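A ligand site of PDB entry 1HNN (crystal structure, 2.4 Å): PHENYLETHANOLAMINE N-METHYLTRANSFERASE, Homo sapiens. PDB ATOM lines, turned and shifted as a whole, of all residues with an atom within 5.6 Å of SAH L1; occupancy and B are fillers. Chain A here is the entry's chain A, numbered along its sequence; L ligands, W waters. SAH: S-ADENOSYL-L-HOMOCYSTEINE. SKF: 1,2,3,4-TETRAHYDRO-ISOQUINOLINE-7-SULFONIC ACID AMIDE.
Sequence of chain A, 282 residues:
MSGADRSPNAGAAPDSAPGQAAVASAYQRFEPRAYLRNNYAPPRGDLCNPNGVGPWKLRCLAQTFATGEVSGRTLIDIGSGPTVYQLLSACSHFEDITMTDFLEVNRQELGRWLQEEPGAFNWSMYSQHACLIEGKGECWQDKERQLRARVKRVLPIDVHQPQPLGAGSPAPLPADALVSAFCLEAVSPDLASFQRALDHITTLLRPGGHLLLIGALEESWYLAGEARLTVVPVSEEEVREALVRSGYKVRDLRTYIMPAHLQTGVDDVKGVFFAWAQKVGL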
ATOM      1  N   VAL A  23      11.315  -0.071  15.973  1.00  0.00           N
ATOM      2  CA  VAL A  23      12.420  -0.976  16.296  1.00  0.00           C
ATOM      3  C   VAL A  23      13.265  -0.235  17.338  1.00  0.00           C
ATOM      4  O   VAL A  23      13.669  -0.804  18.354  1.00  0.00           O
ATOM      5  CB  VAL A  23      13.292  -1.288  15.046  1.00  0.00           C
ATOM      6  CG1 VAL A  23      12.559  -2.259  14.121  1.00  0.00           C
ATOM      7  CG2 VAL A  23      13.638  -0.002  14.290  1.00  0.00           C
ATOM      8  N   ALA A  24      13.492   1.049  17.069  1.00  0.00           N
ATOM      9  CA  ALA A  24      14.280   1.932  17.931  1.00  0.00           C
ATOM     10  C   ALA A  24      13.946   1.722  19.399  1.00  0.00           C
ATOM     11  O   ALA A  24      14.834   1.766  20.257  1.00  0.00           O
ATOM     12  CB  ALA A  24      14.043   3.395  17.539  1.00  0.00           C
ATOM     13  N   TYR A  27      15.740  -1.148  20.317  1.00  0.00           N
ATOM     14  CA  TYR A  27      17.153  -0.777  20.264  1.00  0.00           C
ATOM     15  C   TYR A  27      17.571   0.076  21.453  1.00  0.00           C
ATOM     16  O   TYR A  27      18.759   0.354  21.630  1.00  0.00           O
ATOM     17  CB  TYR A  27      17.482  -0.041  18.971  1.00  0.00           C
ATOM     18  CG  TYR A  27      17.861  -0.981  17.846  1.00  0.00           C
ATOM     19  CD1 TYR A  27      16.986  -1.212  16.782  1.00  0.00           C
ATOM     20  CD2 TYR A  27      19.070  -1.683  17.869  1.00  0.00           C
ATOM     21  CE1 TYR A  27      17.312  -2.123  15.770  1.00  0.00           C
ATOM     22  CE2 TYR A  27      19.407  -2.588  16.870  1.00  0.00           C
ATOM     23  CZ  TYR A  27      18.521  -2.807  15.834  1.00  0.00           C
ATOM     24  OH  TYR A  27      18.842  -3.718  14.852  1.00  0.00           O
ATOM     25  N   PHE A  30      19.418  -2.147  23.690  1.00  0.00           N
ATOM     26  CA  PHE A  30      20.595  -2.733  23.028  1.00  0.00           C
ATOM     27  C   PHE A  30      21.870  -2.662  23.878  1.00  0.00           C
ATOM     28  O   PHE A  30      22.315  -1.574  24.234  1.00  0.00           O
ATOM     29  CB  PHE A  30      20.828  -2.005  21.718  1.00  0.00           C
ATOM     30  CG  PHE A  30      21.806  -2.670  20.803  1.00  0.00           C
ATOM     31  CD1 PHE A  30      21.365  -3.612  19.871  1.00  0.00           C
ATOM     32  CD2 PHE A  30      23.148  -2.313  20.818  1.00  0.00           C
ATOM     33  CE1 PHE A  30      22.247  -4.182  18.962  1.00  0.00           C
ATOM     34  CE2 PHE A  30      24.039  -2.864  19.900  1.00  0.00           C
ATOM     35  CZ  PHE A  30      23.588  -3.802  18.967  1.00  0.00           C
ATOM     36  N   TYR A  35      26.176  -7.723  22.405  1.00  0.00           N
ATOM     37  CA  TYR A  35      26.123  -7.915  20.976  1.00  0.00           C
ATOM     38  C   TYR A  35      27.485  -8.478  20.532  1.00  0.00           C
ATOM     39  O   TYR A  35      27.560  -9.540  19.907  1.00  0.00           O
ATOM     40  CB  TYR A  35      25.841  -6.570  20.298  1.00  0.00           C
ATOM     41  CG  TYR A  35      25.880  -6.628  18.798  1.00  0.00           C
ATOM     42  CD1 TYR A  35      24.885  -7.272  18.067  1.00  0.00           C
ATOM     43  CD2 TYR A  35      26.918  -6.028  18.091  1.00  0.00           C
ATOM     44  CE1 TYR A  35      24.929  -7.321  16.680  1.00  0.00           C
ATOM     45  CE2 TYR A  35      26.975  -6.071  16.707  1.00  0.00           C
ATOM     46  CZ  TYR A  35      25.984  -6.719  16.007  1.00  0.00           C
ATOM     47  OH  TYR A  35      26.052  -6.747  14.645  1.00  0.00           O
ATOM     48  N   TYR A  40      31.099 -11.691  17.882  1.00  0.00           N
ATOM     49  CA  TYR A  40      32.495 -11.510  17.536  1.00  0.00           C
ATOM     50  C   TYR A  40      33.491 -12.179  18.466  1.00  0.00           C
ATOM     51  O   TYR A  40      34.690 -11.894  18.411  1.00  0.00           O
ATOM     52  CB  TYR A  40      32.781 -10.026  17.395  1.00  0.00           C
ATOM     53  CG  TYR A  40      31.964  -9.433  16.272  1.00  0.00           C
ATOM     54  CD1 TYR A  40      30.723  -8.840  16.515  1.00  0.00           C
ATOM     55  CD2 TYR A  40      32.407  -9.539  14.947  1.00  0.00           C
ATOM     56  CE1 TYR A  40      29.930  -8.357  15.455  1.00  0.00           C
ATOM     57  CE2 TYR A  40      31.631  -9.063  13.900  1.00  0.00           C
ATOM     58  CZ  TYR A  40      30.407  -8.477  14.156  1.00  0.00           C
ATOM     59  OH  TYR A  40      29.658  -8.020  13.103  1.00  0.00           O
ATOM     60  N   ASP A  77      30.763   4.625   7.014  1.00  0.00           N
ATOM     61  CA  ASP A  77      30.310   3.335   7.516  1.00  0.00           C
ATOM     62  C   ASP A  77      28.969   3.638   8.170  1.00  0.00           C
ATOM     63  O   ASP A  77      28.878   4.467   9.081  1.00  0.00           O
ATOM     64  CB  ASP A  77      31.298   2.778   8.539  1.00  0.00           C
ATOM     65  CG  ASP A  77      30.914   1.370   9.020  1.00  0.00           C
ATOM     66  OD1 ASP A  77      30.633   0.516   8.151  1.00  0.00           O
ATOM     67  OD2 ASP A  77      30.913   1.122  10.234  1.00  0.00           O
ATOM     68  N   ILE A  78      27.924   2.956   7.703  1.00  0.00           N
ATOM     69  CA  ILE A  78      26.565   3.163   8.199  1.00  0.00           C
ATOM     70  C   ILE A  78      26.147   2.141   9.234  1.00  0.00           C
ATOM     71  O   ILE A  78      26.151   0.934   8.958  1.00  0.00           O
ATOM     72  CB  ILE A  78      25.556   3.114   7.044  1.00  0.00           C
ATOM     73  CG1 ILE A  78      25.948   4.146   5.995  1.00  0.00           C
ATOM     74  CG2 ILE A  78      24.159   3.397   7.545  1.00  0.00           C
ATOM     75  CD1 ILE A  78      25.335   3.881   4.663  1.00  0.00           C
ATOM     76  N   GLY A  79      25.762   2.612  10.416  1.00  0.00           N
ATOM     77  CA  GLY A  79      25.351   1.704  11.455  1.00  0.00           C
ATOM     78  C   GLY A  79      26.539   0.823  11.784  1.00  0.00           C
ATOM     79  O   GLY A  79      26.480  -0.402  11.710  1.00  0.00           O
ATOM     80  N   SER A  80      27.630   1.489  12.137  1.00  0.00           N
ATOM     81  CA  SER A  80      28.865   0.812  12.491  1.00  0.00           C
ATOM     82  C   SER A  80      28.624  -0.083  13.694  1.00  0.00           C
ATOM     83  O   SER A  80      29.208  -1.154  13.825  1.00  0.00           O
ATOM     84  CB  SER A  80      29.925   1.849  12.858  1.00  0.00           C
ATOM     85  OG  SER A  80      30.008   2.855  11.863  1.00  0.00           O
ATOM     86  N   GLY A  81      27.731   0.354  14.578  1.00  0.00           N
ATOM     87  CA  GLY A  81      27.476  -0.399  15.782  1.00  0.00           C
ATOM     88  C   GLY A  81      28.741  -0.280  16.600  1.00  0.00           C
ATOM     89  O   GLY A  81      29.433   0.742  16.522  1.00  0.00           O
ATOM     90  N   PRO A  82      29.077  -1.285  17.419  1.00  0.00           N
ATOM     91  CA  PRO A  82      30.309  -1.152  18.211  1.00  0.00           C
ATOM     92  C   PRO A  82      31.496  -1.859  17.558  1.00  0.00           C
ATOM     93  O   PRO A  82      32.507  -2.083  18.208  1.00  0.00           O
ATOM     94  CB  PRO A  82      29.926  -1.818  19.526  1.00  0.00           C
ATOM     95  CG  PRO A  82      29.090  -2.984  19.034  1.00  0.00           C
ATOM     96  CD  PRO A  82      28.222  -2.366  17.943  1.00  0.00           C
ATOM     97  N   THR A  83      31.386  -2.194  16.277  1.00  0.00           N
ATOM     98  CA  THR A  83      32.432  -2.932  15.566  1.00  0.00           C
ATOM     99  C   THR A  83      33.268  -2.141  14.563  1.00  0.00           C
ATOM    100  O   THR A  83      32.809  -1.130  14.026  1.00  0.00           O
ATOM    101  CB  THR A  83      31.817  -4.141  14.830  1.00  0.00           C
ATOM    102  OG1 THR A  83      31.132  -3.684  13.656  1.00  0.00           O
ATOM    103  CG2 THR A  83      30.815  -4.867  15.743  1.00  0.00           C
ATOM    104  N   TYR A  85      35.738  -4.131  12.333  1.00  0.00           N
ATOM    105  CA  TYR A  85      36.281  -5.077  11.361  1.00  0.00           C
ATOM    106  C   TYR A  85      35.924  -4.740   9.919  1.00  0.00           C
ATOM    107  O   TYR A  85      36.690  -5.036   9.006  1.00  0.00           O
ATOM    108  CB  TYR A  85      35.778  -6.491  11.656  1.00  0.00           C
ATOM    109  CG  TYR A  85      34.323  -6.690  11.259  1.00  0.00           C
ATOM    110  CD1 TYR A  85      33.984  -7.149   9.993  1.00  0.00           C
ATOM    111  CD2 TYR A  85      33.298  -6.355  12.135  1.00  0.00           C
ATOM    112  CE1 TYR A  85      32.659  -7.255   9.601  1.00  0.00           C
ATOM    113  CE2 TYR A  85      31.960  -6.458  11.762  1.00  0.00           C
ATOM    114  CZ  TYR A  85      31.657  -6.908  10.493  1.00  0.00           C
ATOM    115  OH  TYR A  85      30.348  -6.989  10.115  1.00  0.00           O
ATOM    116  N   GLN A  86      34.762  -4.144   9.719  1.00  0.00           N
ATOM    117  CA  GLN A  86      34.300  -3.812   8.371  1.00  0.00           C
ATOM    118  C   GLN A  86      35.104  -2.719   7.674  1.00  0.00           C
ATOM    119  O   GLN A  86      34.906  -2.479   6.474  1.00  0.00           O
ATOM    120  CB  GLN A  86      32.835  -3.423   8.435  1.00  0.00           C
ATOM    121  CG  GLN A  86      32.233  -3.680   9.801  1.00  0.00           C
ATOM    122  CD  GLN A  86      32.208  -2.432  10.644  1.00  0.00           C
ATOM    123  OE1 GLN A  86      32.090  -2.492  11.862  1.00  0.00           O
ATOM    124  NE2 GLN A  86      32.291  -1.288   9.988  1.00  0.00           N
ATOM    125  N   ASP A 101      26.269   5.584  13.754  1.00  0.00           N
ATOM    126  CA  ASP A 101      25.338   4.754  14.485  1.00  0.00           C
ATOM    127  C   ASP A 101      24.260   5.488  15.251  1.00  0.00           C
ATOM    128  O   ASP A 101      24.493   6.517  15.891  1.00  0.00           O
ATOM    129  CB  ASP A 101      26.035   3.795  15.423  1.00  0.00           C
ATOM    130  CG  ASP A 101      25.149   2.625  15.756  1.00  0.00           C
ATOM    131  OD1 ASP A 101      24.900   1.784  14.853  1.00  0.00           O
ATOM    132  OD2 ASP A 101      24.665   2.560  16.906  1.00  0.00           O
ATOM    133  N   PHE A 102      23.057   4.942  15.165  1.00  0.00           N
ATOM    134  CA  PHE A 102      21.865   5.482  15.813  1.00  0.00           C
ATOM    135  C   PHE A 102      21.997   5.607  17.336  1.00  0.00           C
ATOM    136  O   PHE A 102      21.649   6.638  17.920  1.00  0.00           O
ATOM    137  CB  PHE A 102      20.667   4.598  15.445  1.00  0.00           C
ATOM    138  CG  PHE A 102      19.361   5.042  16.058  1.00  0.00           C
ATOM    139  CD1 PHE A 102      18.704   6.177  15.611  1.00  0.00           C
ATOM    140  CD2 PHE A 102      18.784   4.298  17.091  1.00  0.00           C
ATOM    141  CE1 PHE A 102      17.490   6.583  16.179  1.00  0.00           C
ATOM    142  CE2 PHE A 102      17.561   4.685  17.668  1.00  0.00           C
ATOM    143  CZ  PHE A 102      16.919   5.825  17.213  1.00  0.00           C
ATOM    144  N   LEU A 103      22.510   4.557  17.973  1.00  0.00           N
ATOM    145  CA  LEU A 103      22.657   4.544  19.435  1.00  0.00           C
ATOM    146  C   LEU A 103      23.922   5.210  19.963  1.00  0.00           C
ATOM    147  O   LEU A 103      25.021   4.965  19.458  1.00  0.00           O
ATOM    148  CB  LEU A 103      22.622   3.109  19.960  1.00  0.00           C
ATOM    149  CG  LEU A 103      21.281   2.382  19.925  1.00  0.00           C
ATOM    150  CD1 LEU A 103      21.471   0.909  20.257  1.00  0.00           C
ATOM    151  CD2 LEU A 103      20.363   3.051  20.932  1.00  0.00           C
ATOM    152  N   ASN A 106      26.634   2.745  21.377  1.00  0.00           N
ATOM    153  CA  ASN A 106      27.585   2.198  20.430  1.00  0.00           C
ATOM    154  C   ASN A 106      28.650   3.224  20.075  1.00  0.00           C
ATOM    155  O   ASN A 106      29.836   2.907  20.155  1.00  0.00           O
ATOM    156  CB  ASN A 106      26.884   1.693  19.167  1.00  0.00           C
ATOM    157  CG  ASN A 106      26.149   0.385  19.402  1.00  0.00           C
ATOM    158  OD1 ASN A 106      26.532  -0.408  20.266  1.00  0.00           O
ATOM    159  ND2 ASN A 106      25.099   0.135  18.621  1.00  0.00           N
ATOM    160  N   ILE A 157      23.279   8.623  13.372  1.00  0.00           N
ATOM    161  CA  ILE A 157      22.611   8.501  12.085  1.00  0.00           C
ATOM    162  C   ILE A 157      21.288   7.740  12.246  1.00  0.00           C
ATOM    163  O   ILE A 157      21.075   7.033  13.245  1.00  0.00           O
ATOM    164  CB  ILE A 157      23.533   7.757  11.086  1.00  0.00           C
ATOM    165  CG1 ILE A 157      22.902   7.716   9.696  1.00  0.00           C
ATOM    166  CG2 ILE A 157      23.789   6.341  11.584  1.00  0.00           C
ATOM    167  CD1 ILE A 157      23.781   7.065   8.641  1.00  0.00           C
ATOM    168  N   ASP A 158      20.405   7.918  11.263  1.00  0.00           N
ATOM    169  CA  ASP A 158      19.106   7.274  11.218  1.00  0.00           C
ATOM    170  C   ASP A 158      18.763   7.013   9.763  1.00  0.00           C
ATOM    171  O   ASP A 158      18.444   7.944   9.006  1.00  0.00           O
ATOM    172  CB  ASP A 158      18.023   8.175  11.803  1.00  0.00           C
ATOM    173  CG  ASP A 158      16.679   7.465  11.942  1.00  0.00           C
ATOM    174  OD1 ASP A 158      16.407   6.526  11.154  1.00  0.00           O
ATOM    175  OD2 ASP A 158      15.905   7.850  12.836  1.00  0.00           O
ATOM    176  N   VAL A 159      18.836   5.752   9.356  1.00  0.00           N
ATOM    177  CA  VAL A 159      18.561   5.410   7.963  1.00  0.00           C
ATOM    178  C   VAL A 159      17.088   5.619   7.583  1.00  0.00           C
ATOM    179  O   VAL A 159      16.730   5.603   6.407  1.00  0.00           O
ATOM    180  CB  VAL A 159      18.985   3.946   7.657  1.00  0.00           C
ATOM    181  CG1 VAL A 159      20.500   3.829   7.803  1.00  0.00           C
ATOM    182  CG2 VAL A 159      18.289   2.974   8.600  1.00  0.00           C
ATOM    183  N   HIS A 160      16.251   5.824   8.593  1.00  0.00           N
ATOM    184  CA  HIS A 160      14.824   6.025   8.364  1.00  0.00           C
ATOM    185  C   HIS A 160      14.500   7.450   7.904  1.00  0.00           C
ATOM    186  O   HIS A 160      13.452   7.674   7.278  1.00  0.00           O
ATOM    187  CB  HIS A 160      14.058   5.684   9.637  1.00  0.00           C
ATOM    188  CG  HIS A 160      14.152   4.229  10.002  1.00  0.00           C
ATOM    189  ND1 HIS A 160      14.129   3.781  11.298  1.00  0.00           N
ATOM    190  CD2 HIS A 160      14.253   3.131   9.218  1.00  0.00           C
ATOM    191  CE1 HIS A 160      14.226   2.463  11.311  1.00  0.00           C
ATOM    192  NE2 HIS A 160      14.296   2.043  10.062  1.00  0.00           N
ATOM    193  N   ALA A 181      27.220  -2.968   7.373  1.00  0.00           N
ATOM    194  CA  ALA A 181      27.144  -4.368   7.779  1.00  0.00           C
ATOM    195  C   ALA A 181      26.063  -4.622   8.813  1.00  0.00           C
ATOM    196  O   ALA A 181      26.038  -3.988   9.873  1.00  0.00           O
ATOM    197  CB  ALA A 181      28.514  -4.843   8.326  1.00  0.00           C
ATOM    198  N   PHE A 182      25.161  -5.549   8.509  1.00  0.00           N
ATOM    199  CA  PHE A 182      24.064  -5.922   9.394  1.00  0.00           C
ATOM    200  C   PHE A 182      23.251  -4.739   9.936  1.00  0.00           C
ATOM    201  O   PHE A 182      22.854  -4.730  11.104  1.00  0.00           O
ATOM    202  CB  PHE A 182      24.594  -6.750  10.569  1.00  0.00           C
ATOM    203  CG  PHE A 182      25.460  -7.909  10.149  1.00  0.00           C
ATOM    204  CD1 PHE A 182      26.853  -7.775  10.086  1.00  0.00           C
ATOM    205  CD2 PHE A 182      24.893  -9.126   9.797  1.00  0.00           C
ATOM    206  CE1 PHE A 182      27.659  -8.830   9.668  1.00  0.00           C
ATOM    207  CE2 PHE A 182      25.695 -10.190   9.379  1.00  0.00           C
ATOM    208  CZ  PHE A 182      27.073 -10.040   9.313  1.00  0.00           C
ATOM    209  N   CYS A 183      22.977  -3.743   9.108  1.00  0.00           N
ATOM    210  CA  CYS A 183      22.199  -2.609   9.594  1.00  0.00           C
ATOM    211  C   CYS A 183      20.777  -2.583   9.045  1.00  0.00           C
ATOM    212  O   CYS A 183      19.820  -2.852   9.776  1.00  0.00           O
ATOM    213  CB  CYS A 183      22.881  -1.294   9.247  1.00  0.00           C
ATOM    214  SG  CYS A 183      21.982   0.117   9.942  1.00  0.00           S
ATOM    215  N   ALA A 186      18.221  -5.046   9.939  1.00  0.00           N
ATOM    216  CA  ALA A 186      18.008  -5.145  11.372  1.00  0.00           C
ATOM    217  C   ALA A 186      17.336  -3.907  11.952  1.00  0.00           C
ATOM    218  O   ALA A 186      17.082  -3.845  13.158  1.00  0.00           O
ATOM    219  CB  ALA A 186      19.338  -5.387  12.071  1.00  0.00           C
ATOM    220  N   VAL A 187      17.051  -2.927  11.101  1.00  0.00           N
ATOM    221  CA  VAL A 187      16.409  -1.699  11.554  1.00  0.00           C
ATOM    222  C   VAL A 187      15.088  -1.447  10.827  1.00  0.00           C
ATOM    223  O   VAL A 187      14.360  -0.495  11.145  1.00  0.00           O
ATOM    224  CB  VAL A 187      17.342  -0.474  11.374  1.00  0.00           C
ATOM    225  CG1 VAL A 187      18.645  -0.719  12.098  1.00  0.00           C
ATOM    226  CG2 VAL A 187      17.594  -0.194   9.902  1.00  0.00           C
ATOM    227  N   TYR A 222      17.334 -11.479  16.643  1.00  0.00           N
ATOM    228  CA  TYR A 222      18.676 -11.678  17.172  1.00  0.00           C
ATOM    229  C   TYR A 222      18.716 -10.896  18.472  1.00  0.00           C
ATOM    230  O   TYR A 222      18.166  -9.795  18.572  1.00  0.00           O
ATOM    231  CB  TYR A 222      19.765 -11.197  16.186  1.00  0.00           C
ATOM    232  CG  TYR A 222      19.976  -9.704  16.123  1.00  0.00           C
ATOM    233  CD1 TYR A 222      20.754  -9.048  17.069  1.00  0.00           C
ATOM    234  CD2 TYR A 222      19.414  -8.953  15.093  1.00  0.00           C
ATOM    235  CE1 TYR A 222      20.966  -7.681  16.992  1.00  0.00           C
ATOM    236  CE2 TYR A 222      19.615  -7.592  15.004  1.00  0.00           C
ATOM    237  CZ  TYR A 222      20.391  -6.968  15.958  1.00  0.00           C
ATOM    238  OH  TYR A 222      20.585  -5.603  15.858  1.00  0.00           O
HETATM  239  N   SAH L   1      27.493  -2.914  11.739  1.00  0.00           N
HETATM  240  CA  SAH L   1      27.426  -3.833  12.883  1.00  0.00           C
HETATM  241  CB  SAH L   1      26.043  -4.488  12.923  1.00  0.00           C
HETATM  242  CG  SAH L   1      24.854  -3.582  13.022  1.00  0.00           C
HETATM  243  SD  SAH L   1      23.746  -4.052  14.320  1.00  0.00           S
HETATM  244  C   SAH L   1      28.365  -5.001  12.761  1.00  0.00           C
HETATM  245  O   SAH L   1      28.967  -5.151  11.668  1.00  0.00           O
HETATM  246  OXT SAH L   1      28.409  -5.833  13.693  1.00  0.00           O
HETATM  247  C5' SAH L   1      22.493  -2.810  13.998  1.00  0.00           C
HETATM  248  C4' SAH L   1      22.892  -1.407  14.211  1.00  0.00           C
HETATM  249  O4' SAH L   1      21.699  -0.693  13.877  1.00  0.00           O
HETATM  250  C3' SAH L   1      23.265  -1.034  15.725  1.00  0.00           C
HETATM  251  O3' SAH L   1      24.598  -0.471  15.958  1.00  0.00           O
HETATM  252  C2' SAH L   1      22.098  -0.080  16.033  1.00  0.00           C
HETATM  253  O2' SAH L   1      22.301   0.890  17.093  1.00  0.00           O
HETATM  254  C1' SAH L   1      21.814   0.483  14.632  1.00  0.00           C
HETATM  255  N9  SAH L   1      20.549   1.182  14.375  1.00  0.00           N
HETATM  256  C8  SAH L   1      19.313   1.094  15.099  1.00  0.00           C
HETATM  257  N7  SAH L   1      18.410   1.854  14.555  1.00  0.00           N
HETATM  258  C5  SAH L   1      19.024   2.486  13.455  1.00  0.00           C
HETATM  259  C6  SAH L   1      18.572   3.410  12.459  1.00  0.00           C
HETATM  260  N6  SAH L   1      17.334   3.895  12.466  1.00  0.00           N
HETATM  261  N1  SAH L   1      19.431   3.852  11.471  1.00  0.00           N
HETATM  262  C2  SAH L   1      20.686   3.359  11.477  1.00  0.00           C
HETATM  263  N3  SAH L   1      21.233   2.489  12.349  1.00  0.00           N
HETATM  264  C4  SAH L   1      20.341   2.070  13.322  1.00  0.00           C
HETATM  265  C4  SKF L   2      26.549  -9.758  12.988  1.00  0.00           C
HETATM  266  C5  SKF L   2      27.590 -10.628  12.700  1.00  0.00           C
HETATM  267  C6  SKF L   2      27.337 -11.991  12.535  1.00  0.00           C
HETATM  268  C7  SKF L   2      26.036 -12.469  12.657  1.00  0.00           C
HETATM  269  S   SKF L   2      28.648 -13.106  12.179  1.00  0.00           S
HETATM  270  C8  SKF L   2      24.990 -11.608  12.944  1.00  0.00           C
HETATM  271  C9  SKF L   2      25.244 -10.245  13.109  1.00  0.00           C
HETATM  272  O1  SKF L   2      29.914 -12.585  12.652  1.00  0.00           O
HETATM  273  O2  SKF L   2      28.767 -13.402  10.779  1.00  0.00           O
HETATM  274  N   SKF L   2      28.336 -14.447  12.940  1.00  0.00           N
HETATM  275  C1  SKF L   2      23.586 -12.140  12.994  1.00  0.00           C
HETATM  276  C2  SKF L   2      22.841  -9.770  13.174  1.00  0.00           C
HETATM  277  C3  SKF L   2      24.187  -9.377  13.719  1.00  0.00           C
HETATM  278  N1  SKF L   2      22.616 -11.184  13.593  1.00  0.00           N
HETATM  279  O   HOH W   1      22.268  -6.659  13.080  1.00  0.00           O
HETATM  280  O   HOH W   2      14.551   3.208  14.403  1.00  0.00           O
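An oxygen (O3') of SAH L1 sits at hydrogen-bond distance from the side-chain carboxylate (OD1) of Asp 101 (2.5 Å).
OH of Tyr 40 sits at hydrogen-bond distance from OXT of SAH L1, at 2.6 Å.
N of SAH L1 is in hydrogen-bond range of O of Ala 181 (2.6 Å).
The side-chain hydroxyl (OH) of Tyr 35 is in hydrogen-bond range of an oxygen (OXT) of SAH L1, at 2.7 Å.
The backbone carbonyl oxygen of Gly 79 is in hydrogen-bond range of a nitrogen (N) of SAH L1, 2.7 Å away.
OH of Tyr 85 lies within hydrogen-bond range of O of SAH L1 (2.8 Å).
An oxygen (O3') of SAH L1 sits at hydrogen-bond distance from the side-chain amide nitrogen (ND2) of Asn 106 (2.8 Å).
N of Val 159 sits at hydrogen-bond distance from N1 of SAH L1 (2.9 Å).
OD1 of Asp 158 is in hydrogen-bond range of N6 of SAH L1 (3.1 Å).
An oxygen (O) of SAH L1 lies close to the side-chain hydroxyl (OG1) of Thr 83.
The backbone carbonyl oxygen (O) of Ser 80 sits at hydrogen-bond distance from a nitrogen (N) of SAH L1, at 3.2 Å.
A nitrogen (N6) of SAH L1 lies within hydrogen-bond range of a ring nitrogen (ND1) of His 160 (3.4 Å).
A nitrogen (N3) of SAH L1 sits at hydrogen-bond distance from the side-chain sulfur (SG) of Cys 183 (3.5 Å).
The side-chain amide nitrogen (ND2) of Asn 106 is in hydrogen-bond range of the side-chain carboxylate (OD2) of Asp 101, 3.0 Å away.
OD1 of Asp 101 sits at hydrogen-bond distance from N of Gly 81.
OD2 of Asp 101 sits at hydrogen-bond distance from N of Leu 103, 3.1 Å away.
The side-chain hydroxyl (OG1) of Thr 83 is in hydrogen-bond range of the backbone carbonyl oxygen (O) of Ser 80, 3.2 Å away.
The backbone carbonyl oxygen (O) of Thr 83 lies close to the side-chain amide oxygen (OE1) of Gln 86, at 2.7 Å.
The side-chain hydroxyl of Ser 80 sits at hydrogen-bond distance from the side-chain carboxylate of Asp 77 (2.5 Å).
O of Val 187 sits at hydrogen-bond distance from NE2 of His 160 (2.8 Å).
The side-chain hydroxyl (OH) of Tyr 27 sits at hydrogen-bond distance from the side-chain hydroxyl (OH) of Tyr 222 (2.8 Å).
SD of SAH L1 lies close to O of Phe 182 (3.4 Å).
CD1 of Tyr 27 touches C8 of SAH L1, at 3.7 Å.
CA of Gly 81 touches O3' of SAH L1, 2.9 Å away.
Phe 102 touches SAH L1 (CB to C4, 3.3 Å).
Leu 103 touches SAH L1 (CD1 to O2', 3.3 Å).
Ile 157 touches SAH L1.
Val 187 touches SAH L1 (CG1 to C4, 3.5 Å).
Tyr 222 touches SAH L1 (OH to SD, 3.8 Å).
Hydrophobic or aromatic side chains that line SAH L1: Tyr 27, Tyr 35, Tyr 40, Tyr 85, Phe 102, Leu 103, Val 159, His 160, Ala 181, Phe 182 and Val 187.
21 residues have an atom within 4 Å of SAH L1: Tyr 27, Tyr 35, Tyr 40, Gly 79, Ser 80, Gly 81, Thr 83, Tyr 85, Asp 101, Phe 102, Leu 103, Asn 106, Ile 157, Asp 158, Val 159, His 160, Ala 181, Phe 182, Cys 183, Val 187 and Tyr 222.
The nearest printed residue that does not touch SAH L1 is Gln 86 (4.04 Å).
Water W1 lies within hydrogen-bond range of the backbone carbonyl oxygen (O) of Phe 182 (2.8 Å), a sulfur (SD) of SAH L1 (3.2 Å) and the side-chain hydroxyl (OH) of Tyr 222 (3.4 Å).
Water W2 lies within hydrogen-bond range of ND1 of His 160 (3.2 Å) and N6 of SAH L1 (3.5 Å).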
